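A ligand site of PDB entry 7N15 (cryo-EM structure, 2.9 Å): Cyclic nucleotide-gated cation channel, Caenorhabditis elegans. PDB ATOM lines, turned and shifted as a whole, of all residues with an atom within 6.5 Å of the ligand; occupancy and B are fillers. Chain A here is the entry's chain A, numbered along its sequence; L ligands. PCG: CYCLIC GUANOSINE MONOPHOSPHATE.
Residues that only touch the ligand: Cys 526 (3.98 Å), Val 555 (3.8 Å), Phe 563 (3.4 Å), Glu 565 (3.9 Å), Leu 566 (3.4 Å), Ala 582 (3.6 Å) and Val 584 (3.8 Å). Hydrophobic or aromatic side chains that line the ligand: Val 555, Phe 563, Leu 566, Ala 582 and Val 584.
The backbone carbonyl oxygen (O) of Gly 564 sits at hydrogen-bond distance from the guanidinium group (NH1) of Arg 580, at 2.9 Å. SG of Cys 526 lies within hydrogen-bond range of NE of Arg 580 (3.8 Å). The guanidinium group (NH2) of Arg 580 sits at hydrogen-bond distance from the backbone carbonyl oxygen (O) of Glu 534, 3.1 Å away. N of Gly 532 is in hydrogen-bond range of OG of Ser 567 (3.2 Å). N of Val 584 lies within hydrogen-bond range of O of Cys 526, at 3.0 Å. N of Val 545 sits at hydrogen-bond distance from O of Val 555 (2.9 Å).
The backbone NH (N) of Thr 581 lies within hydrogen-bond range of an oxygen (O1A) of the ligand (2.6 Å). A nitrogen (N2) of the ligand is in hydrogen-bond range of the side-chain hydroxyl (OG1) of Thr 581 (2.8 Å). A nitrogen (N2) of the ligand sits at hydrogen-bond distance from the side-chain carboxylate (OD2) of Asp 625 (2.8 Å). An oxygen (O2A) of the ligand is in salt-bridge range of the guanidinium group (NH1) of Arg 580, at 2.9 Å. An oxygen (O2') of the ligand lies within hydrogen-bond range of the backbone NH (N) of Gly 564. The backbone NH (N) of Ser 567 lies within hydrogen-bond range of an oxygen (O2A) of the ligand (3.2 Å).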
ATOM      1  N   CYS A 526     -31.596   6.686 -25.865  1.00  0.00           N
ATOM      2  CA  CYS A 526     -30.787   7.376 -26.851  1.00  0.00           C
ATOM      3  C   CYS A 526     -30.030   6.353 -27.674  1.00  0.00           C
ATOM      4  O   CYS A 526     -29.515   5.378 -27.128  1.00  0.00           O
ATOM      5  CB  CYS A 526     -29.781   8.327 -26.201  1.00  0.00           C
ATOM      6  SG  CYS A 526     -30.467   9.459 -24.995  1.00  0.00           S
ATOM      7  N   LYS A 527     -29.953   6.585 -28.983  1.00  0.00           N
ATOM      8  CA  LYS A 527     -28.969   5.879 -29.805  1.00  0.00           C
ATOM      9  C   LYS A 527     -28.475   6.820 -30.890  1.00  0.00           C
ATOM     10  O   LYS A 527     -29.114   7.834 -31.184  1.00  0.00           O
ATOM     11  CB  LYS A 527     -29.522   4.566 -30.382  1.00  0.00           C
ATOM     12  CG  LYS A 527     -30.736   4.666 -31.267  1.00  0.00           C
ATOM     13  CD  LYS A 527     -31.129   3.265 -31.708  1.00  0.00           C
ATOM     14  CE  LYS A 527     -32.377   3.270 -32.553  1.00  0.00           C
ATOM     15  NZ  LYS A 527     -33.544   3.639 -31.730  1.00  0.00           N
ATOM     16  N   GLY A 532     -31.291  14.597 -30.937  1.00  0.00           N
ATOM     17  CA  GLY A 532     -31.672  14.817 -29.561  1.00  0.00           C
ATOM     18  C   GLY A 532     -32.213  16.203 -29.275  1.00  0.00           C
ATOM     19  O   GLY A 532     -31.573  17.207 -29.560  1.00  0.00           O
ATOM     20  N   GLU A 534     -33.696  16.630 -26.047  1.00  0.00           N
ATOM     21  CA  GLU A 534     -33.967  16.526 -24.622  1.00  0.00           C
ATOM     22  C   GLU A 534     -32.730  16.030 -23.888  1.00  0.00           C
ATOM     23  O   GLU A 534     -31.875  15.360 -24.467  1.00  0.00           O
ATOM     24  CB  GLU A 534     -35.122  15.563 -24.358  1.00  0.00           C
ATOM     25  CG  GLU A 534     -36.509  16.115 -24.648  1.00  0.00           C
ATOM     26  CD  GLU A 534     -37.537  15.020 -24.817  1.00  0.00           C
ATOM     27  OE1 GLU A 534     -37.136  13.869 -25.049  1.00  0.00           O
ATOM     28  OE2 GLU A 534     -38.745  15.307 -24.672  1.00  0.00           O
ATOM     29  N   VAL A 545     -24.650   2.273 -20.939  1.00  0.00           N
ATOM     30  CA  VAL A 545     -24.160   2.847 -22.187  1.00  0.00           C
ATOM     31  C   VAL A 545     -23.529   1.724 -23.002  1.00  0.00           C
ATOM     32  O   VAL A 545     -22.453   1.215 -22.649  1.00  0.00           O
ATOM     33  CB  VAL A 545     -23.178   3.989 -21.928  1.00  0.00           C
ATOM     34  CG1 VAL A 545     -22.771   4.623 -23.231  1.00  0.00           C
ATOM     35  CG2 VAL A 545     -23.808   5.020 -21.030  1.00  0.00           C
ATOM     36  N   PHE A 554     -20.082   0.202 -21.559  1.00  0.00           N
ATOM     37  CA  PHE A 554     -19.002   1.102 -21.172  1.00  0.00           C
ATOM     38  C   PHE A 554     -19.150   1.563 -19.730  1.00  0.00           C
ATOM     39  O   PHE A 554     -18.252   1.348 -18.909  1.00  0.00           O
ATOM     40  CB  PHE A 554     -18.939   2.327 -22.072  1.00  0.00           C
ATOM     41  CG  PHE A 554     -18.479   2.040 -23.456  1.00  0.00           C
ATOM     42  CD1 PHE A 554     -17.405   1.178 -23.678  1.00  0.00           C
ATOM     43  CD2 PHE A 554     -19.060   2.668 -24.546  1.00  0.00           C
ATOM     44  CE1 PHE A 554     -16.954   0.915 -24.956  1.00  0.00           C
ATOM     45  CE2 PHE A 554     -18.610   2.429 -25.819  1.00  0.00           C
ATOM     46  CZ  PHE A 554     -17.553   1.543 -26.028  1.00  0.00           C
ATOM     47  N   VAL A 555     -20.278   2.185 -19.416  1.00  0.00           N
ATOM     48  CA  VAL A 555     -20.517   2.745 -18.093  1.00  0.00           C
ATOM     49  C   VAL A 555     -22.011   2.635 -17.793  1.00  0.00           C
ATOM     50  O   VAL A 555     -22.846   2.741 -18.702  1.00  0.00           O
ATOM     51  CB  VAL A 555     -19.976   4.204 -18.008  1.00  0.00           C
ATOM     52  CG1 VAL A 555     -20.660   5.144 -19.002  1.00  0.00           C
ATOM     53  CG2 VAL A 555     -20.045   4.755 -16.576  1.00  0.00           C
ATOM     54  N   LEU A 557     -25.449   3.834 -15.551  1.00  0.00           N
ATOM     55  CA  LEU A 557     -26.025   5.086 -15.058  1.00  0.00           C
ATOM     56  C   LEU A 557     -27.030   4.755 -13.970  1.00  0.00           C
ATOM     57  O   LEU A 557     -27.966   3.976 -14.190  1.00  0.00           O
ATOM     58  CB  LEU A 557     -26.680   5.867 -16.191  1.00  0.00           C
ATOM     59  CG  LEU A 557     -25.728   6.344 -17.295  1.00  0.00           C
ATOM     60  CD1 LEU A 557     -26.500   6.958 -18.435  1.00  0.00           C
ATOM     61  CD2 LEU A 557     -24.743   7.337 -16.727  1.00  0.00           C
ATOM     62  N   VAL A 562     -26.721  12.278 -14.961  1.00  0.00           N
ATOM     63  CA  VAL A 562     -27.123  13.231 -15.980  1.00  0.00           C
ATOM     64  C   VAL A 562     -26.576  12.740 -17.310  1.00  0.00           C
ATOM     65  O   VAL A 562     -25.366  12.503 -17.439  1.00  0.00           O
ATOM     66  CB  VAL A 562     -26.627  14.648 -15.669  1.00  0.00           C
ATOM     67  CG1 VAL A 562     -27.039  15.602 -16.751  1.00  0.00           C
ATOM     68  CG2 VAL A 562     -27.165  15.109 -14.333  1.00  0.00           C
ATOM     69  N   PHE A 563     -27.457  12.565 -18.283  1.00  0.00           N
ATOM     70  CA  PHE A 563     -27.047  12.137 -19.618  1.00  0.00           C
ATOM     71  C   PHE A 563     -27.995  12.745 -20.629  1.00  0.00           C
ATOM     72  O   PHE A 563     -29.050  13.262 -20.287  1.00  0.00           O
ATOM     73  CB  PHE A 563     -26.990  10.606 -19.735  1.00  0.00           C
ATOM     74  CG  PHE A 563     -28.329   9.917 -19.688  1.00  0.00           C
ATOM     75  CD1 PHE A 563     -28.958   9.660 -18.477  1.00  0.00           C
ATOM     76  CD2 PHE A 563     -28.950   9.485 -20.861  1.00  0.00           C
ATOM     77  CE1 PHE A 563     -30.182   9.026 -18.442  1.00  0.00           C
ATOM     78  CE2 PHE A 563     -30.176   8.862 -20.818  1.00  0.00           C
ATOM     79  CZ  PHE A 563     -30.787   8.617 -19.606  1.00  0.00           C
ATOM     80  N   GLY A 564     -27.589  12.685 -21.886  1.00  0.00           N
ATOM     81  CA  GLY A 564     -28.386  13.236 -22.955  1.00  0.00           C
ATOM     82  C   GLY A 564     -28.142  14.697 -23.241  1.00  0.00           C
ATOM     83  O   GLY A 564     -28.877  15.284 -24.033  1.00  0.00           O
ATOM     84  N   GLU A 565     -27.127  15.309 -22.623  1.00  0.00           N
ATOM     85  CA  GLU A 565     -26.901  16.727 -22.802  1.00  0.00           C
ATOM     86  C   GLU A 565     -25.948  17.057 -23.938  1.00  0.00           C
ATOM     87  O   GLU A 565     -25.890  18.221 -24.344  1.00  0.00           O
ATOM     88  CB  GLU A 565     -26.365  17.351 -21.503  1.00  0.00           C
ATOM     89  CG  GLU A 565     -24.865  17.204 -21.286  1.00  0.00           C
ATOM     90  CD  GLU A 565     -24.523  16.135 -20.277  1.00  0.00           C
ATOM     91  OE1 GLU A 565     -25.459  15.447 -19.809  1.00  0.00           O
ATOM     92  OE2 GLU A 565     -23.340  15.980 -19.948  1.00  0.00           O
ATOM     93  N   LEU A 566     -25.224  16.065 -24.473  1.00  0.00           N
ATOM     94  CA  LEU A 566     -24.231  16.330 -25.516  1.00  0.00           C
ATOM     95  C   LEU A 566     -24.882  16.736 -26.833  1.00  0.00           C
ATOM     96  O   LEU A 566     -24.277  17.492 -27.603  1.00  0.00           O
ATOM     97  CB  LEU A 566     -23.370  15.086 -25.746  1.00  0.00           C
ATOM     98  CG  LEU A 566     -22.204  14.834 -24.797  1.00  0.00           C
ATOM     99  CD1 LEU A 566     -21.307  13.753 -25.365  1.00  0.00           C
ATOM    100  CD2 LEU A 566     -21.434  16.093 -24.610  1.00  0.00           C
ATOM    101  N   SER A 567     -26.099  16.273 -27.084  1.00  0.00           N
ATOM    102  CA  SER A 567     -26.767  16.612 -28.320  1.00  0.00           C
ATOM    103  C   SER A 567     -27.345  18.017 -28.292  1.00  0.00           C
ATOM    104  O   SER A 567     -27.418  18.673 -29.336  1.00  0.00           O
ATOM    105  CB  SER A 567     -27.886  15.605 -28.595  1.00  0.00           C
ATOM    106  OG  SER A 567     -28.587  15.948 -29.766  1.00  0.00           O
ATOM    107  N   ILE A 568     -27.739  18.509 -27.115  1.00  0.00           N
ATOM    108  CA  ILE A 568     -28.474  19.771 -27.044  1.00  0.00           C
ATOM    109  C   ILE A 568     -27.555  20.915 -26.631  1.00  0.00           C
ATOM    110  O   ILE A 568     -27.851  22.084 -26.905  1.00  0.00           O
ATOM    111  CB  ILE A 568     -29.682  19.654 -26.114  1.00  0.00           C
ATOM    112  CG1 ILE A 568     -29.275  19.141 -24.746  1.00  0.00           C
ATOM    113  CG2 ILE A 568     -30.727  18.740 -26.718  1.00  0.00           C
ATOM    114  CD1 ILE A 568     -30.431  19.097 -23.802  1.00  0.00           C
ATOM    115  N   ARG A 579     -26.384  15.111 -33.142  1.00  0.00           N
ATOM    116  CA  ARG A 579     -26.511  13.673 -33.025  1.00  0.00           C
ATOM    117  C   ARG A 579     -26.233  13.208 -31.593  1.00  0.00           C
ATOM    118  O   ARG A 579     -25.501  13.851 -30.853  1.00  0.00           O
ATOM    119  CB  ARG A 579     -25.538  12.966 -33.963  1.00  0.00           C
ATOM    120  CG  ARG A 579     -25.478  13.547 -35.361  1.00  0.00           C
ATOM    121  CD  ARG A 579     -26.800  13.337 -36.071  1.00  0.00           C
ATOM    122  NE  ARG A 579     -26.809  13.973 -37.384  1.00  0.00           N
ATOM    123  CZ  ARG A 579     -27.855  13.937 -38.199  1.00  0.00           C
ATOM    124  NH1 ARG A 579     -28.952  13.290 -37.831  1.00  0.00           N
ATOM    125  NH2 ARG A 579     -27.803  14.525 -39.387  1.00  0.00           N
ATOM    126  N   ARG A 580     -26.836  12.076 -31.226  1.00  0.00           N
ATOM    127  CA  ARG A 580     -26.451  11.392 -30.008  1.00  0.00           C
ATOM    128  C   ARG A 580     -25.096  10.728 -30.200  1.00  0.00           C
ATOM    129  O   ARG A 580     -24.812  10.167 -31.252  1.00  0.00           O
ATOM    130  CB  ARG A 580     -27.495  10.342 -29.623  1.00  0.00           C
ATOM    131  CG  ARG A 580     -28.898  10.888 -29.422  1.00  0.00           C
ATOM    132  CD  ARG A 580     -28.976  11.728 -28.162  1.00  0.00           C
ATOM    133  NE  ARG A 580     -30.356  11.996 -27.775  1.00  0.00           N
ATOM    134  CZ  ARG A 580     -30.709  12.822 -26.790  1.00  0.00           C
ATOM    135  NH1 ARG A 580     -29.780  13.453 -26.093  1.00  0.00           N
ATOM    136  NH2 ARG A 580     -31.988  13.008 -26.512  1.00  0.00           N
ATOM    137  N   THR A 581     -24.252  10.805 -29.173  1.00  0.00           N
ATOM    138  CA  THR A 581     -22.907  10.249 -29.275  1.00  0.00           C
ATOM    139  C   THR A 581     -22.790   8.850 -28.715  1.00  0.00           C
ATOM    140  O   THR A 581     -21.725   8.230 -28.853  1.00  0.00           O
ATOM    141  CB  THR A 581     -21.906  11.164 -28.557  1.00  0.00           C
ATOM    142  OG1 THR A 581     -21.985  10.961 -27.146  1.00  0.00           O
ATOM    143  CG2 THR A 581     -22.192  12.618 -28.876  1.00  0.00           C
ATOM    144  N   ALA A 582     -23.834   8.316 -28.090  1.00  0.00           N
ATOM    145  CA  ALA A 582     -23.754   7.004 -27.467  1.00  0.00           C
ATOM    146  C   ALA A 582     -25.123   6.353 -27.453  1.00  0.00           C
ATOM    147  O   ALA A 582     -26.144   7.004 -27.703  1.00  0.00           O
ATOM    148  CB  ALA A 582     -23.191   7.092 -26.048  1.00  0.00           C
ATOM    149  N   ASN A 583     -25.133   5.056 -27.167  1.00  0.00           N
ATOM    150  CA  ASN A 583     -26.341   4.241 -27.083  1.00  0.00           C
ATOM    151  C   ASN A 583     -26.597   3.943 -25.604  1.00  0.00           C
ATOM    152  O   ASN A 583     -25.906   3.118 -25.010  1.00  0.00           O
ATOM    153  CB  ASN A 583     -26.198   2.914 -27.854  1.00  0.00           C
ATOM    154  CG  ASN A 583     -25.929   3.124 -29.321  1.00  0.00           C
ATOM    155  OD1 ASN A 583     -26.176   4.177 -29.864  1.00  0.00           O
ATOM    156  ND2 ASN A 583     -25.422   2.082 -29.975  1.00  0.00           N
ATOM    157  N   VAL A 584     -27.578   4.612 -25.014  1.00  0.00           N
ATOM    158  CA  VAL A 584     -27.992   4.219 -23.672  1.00  0.00           C
ATOM    159  C   VAL A 584     -29.209   3.302 -23.752  1.00  0.00           C
ATOM    160  O   VAL A 584     -29.993   3.331 -24.710  1.00  0.00           O
ATOM    161  CB  VAL A 584     -28.256   5.446 -22.762  1.00  0.00           C
ATOM    162  CG1 VAL A 584     -27.063   6.388 -22.791  1.00  0.00           C
ATOM    163  CG2 VAL A 584     -29.516   6.166 -23.148  1.00  0.00           C
ATOM    164  N   ILE A 621     -15.704  14.972 -22.111  1.00  0.00           N
ATOM    165  CA  ILE A 621     -16.051  13.606 -22.523  1.00  0.00           C
ATOM    166  C   ILE A 621     -16.079  13.470 -24.036  1.00  0.00           C
ATOM    167  O   ILE A 621     -15.848  12.378 -24.578  1.00  0.00           O
ATOM    168  CB  ILE A 621     -17.370  13.125 -21.875  1.00  0.00           C
ATOM    169  CG1 ILE A 621     -18.572  13.917 -22.357  1.00  0.00           C
ATOM    170  CG2 ILE A 621     -17.271  13.176 -20.360  1.00  0.00           C
ATOM    171  CD1 ILE A 621     -19.889  13.315 -21.926  1.00  0.00           C
ATOM    172  N   LEU A 622     -16.276  14.572 -24.765  1.00  0.00           N
ATOM    173  CA  LEU A 622     -16.220  14.500 -26.216  1.00  0.00           C
ATOM    174  C   LEU A 622     -14.793  14.391 -26.734  1.00  0.00           C
ATOM    175  O   LEU A 622     -14.557  13.773 -27.774  1.00  0.00           O
ATOM    176  CB  LEU A 622     -16.907  15.717 -26.831  1.00  0.00           C
ATOM    177  CG  LEU A 622     -18.375  15.582 -27.237  1.00  0.00           C
ATOM    178  CD1 LEU A 622     -18.834  16.789 -28.028  1.00  0.00           C
ATOM    179  CD2 LEU A 622     -18.593  14.319 -28.034  1.00  0.00           C
ATOM    180  N   LYS A 624     -12.122  12.947 -24.924  1.00  0.00           N
ATOM    181  CA  LYS A 624     -11.605  11.594 -24.781  1.00  0.00           C
ATOM    182  C   LYS A 624     -12.373  10.590 -25.641  1.00  0.00           C
ATOM    183  O   LYS A 624     -11.887   9.485 -25.904  1.00  0.00           O
ATOM    184  CB  LYS A 624     -11.664  11.103 -23.323  1.00  0.00           C
ATOM    185  CG  LYS A 624     -13.043  10.972 -22.671  1.00  0.00           C
ATOM    186  CD  LYS A 624     -13.021  10.451 -21.221  1.00  0.00           C
ATOM    187  CE  LYS A 624     -14.440  10.360 -20.667  1.00  0.00           C
ATOM    188  NZ  LYS A 624     -14.457   9.858 -19.264  1.00  0.00           N
ATOM    189  N   ASP A 625     -13.561  10.978 -26.105  1.00  0.00           N
ATOM    190  CA  ASP A 625     -14.327  10.154 -27.032  1.00  0.00           C
ATOM    191  C   ASP A 625     -14.089  10.676 -28.440  1.00  0.00           C
ATOM    192  O   ASP A 625     -12.949  10.837 -28.864  1.00  0.00           O
ATOM    193  CB  ASP A 625     -15.826  10.076 -26.751  1.00  0.00           C
ATOM    194  CG  ASP A 625     -16.489   8.877 -27.390  1.00  0.00           C
ATOM    195  OD1 ASP A 625     -15.762   8.031 -27.959  1.00  0.00           O
ATOM    196  OD2 ASP A 625     -17.731   8.781 -27.337  1.00  0.00           O
HETATM  197  PA  PCG L   1     -25.947  12.282 -25.948  1.00  0.00           P
HETATM  198  O1A PCG L   1     -24.978  12.039 -27.027  1.00  0.00           O
HETATM  199  O2A PCG L   1     -26.907  13.385 -26.092  1.00  0.00           O
HETATM  200  O5' PCG L   1     -26.787  10.902 -25.711  1.00  0.00           O
HETATM  201  C5' PCG L   1     -26.123   9.765 -25.112  1.00  0.00           C
HETATM  202  C4' PCG L   1     -25.431  10.229 -23.820  1.00  0.00           C
HETATM  203  O4' PCG L   1     -24.646   9.257 -23.115  1.00  0.00           O
HETATM  204  C3' PCG L   1     -24.423  11.295 -24.108  1.00  0.00           C
HETATM  205  O3' PCG L   1     -25.115  12.447 -24.547  1.00  0.00           O
HETATM  206  C2' PCG L   1     -23.797  11.484 -22.765  1.00  0.00           C
HETATM  207  O2' PCG L   1     -24.576  12.378 -21.994  1.00  0.00           O
HETATM  208  C1' PCG L   1     -23.910  10.075 -22.132  1.00  0.00           C
HETATM  209  N9  PCG L   1     -22.591   9.463 -21.844  1.00  0.00           N
HETATM  210  C8  PCG L   1     -22.237   9.051 -20.619  1.00  0.00           C
HETATM  211  N7  PCG L   1     -20.998   8.558 -20.669  1.00  0.00           N
HETATM  212  C5  PCG L   1     -20.562   8.642 -21.915  1.00  0.00           C
HETATM  213  C6  PCG L   1     -19.359   8.287 -22.512  1.00  0.00           C
HETATM  214  O6  PCG L   1     -18.470   7.775 -21.851  1.00  0.00           O
HETATM  215  N1  PCG L   1     -19.182   8.511 -23.886  1.00  0.00           N
HETATM  216  C2  PCG L   1     -20.236   9.099 -24.612  1.00  0.00           C
HETATM  217  N2  PCG L   1     -20.091   9.318 -25.908  1.00  0.00           N
HETATM  218  N3  PCG L   1     -21.386   9.431 -23.993  1.00  0.00           N
HETATM  219  C4  PCG L   1     -21.573   9.222 -22.664  1.00  0.00           C
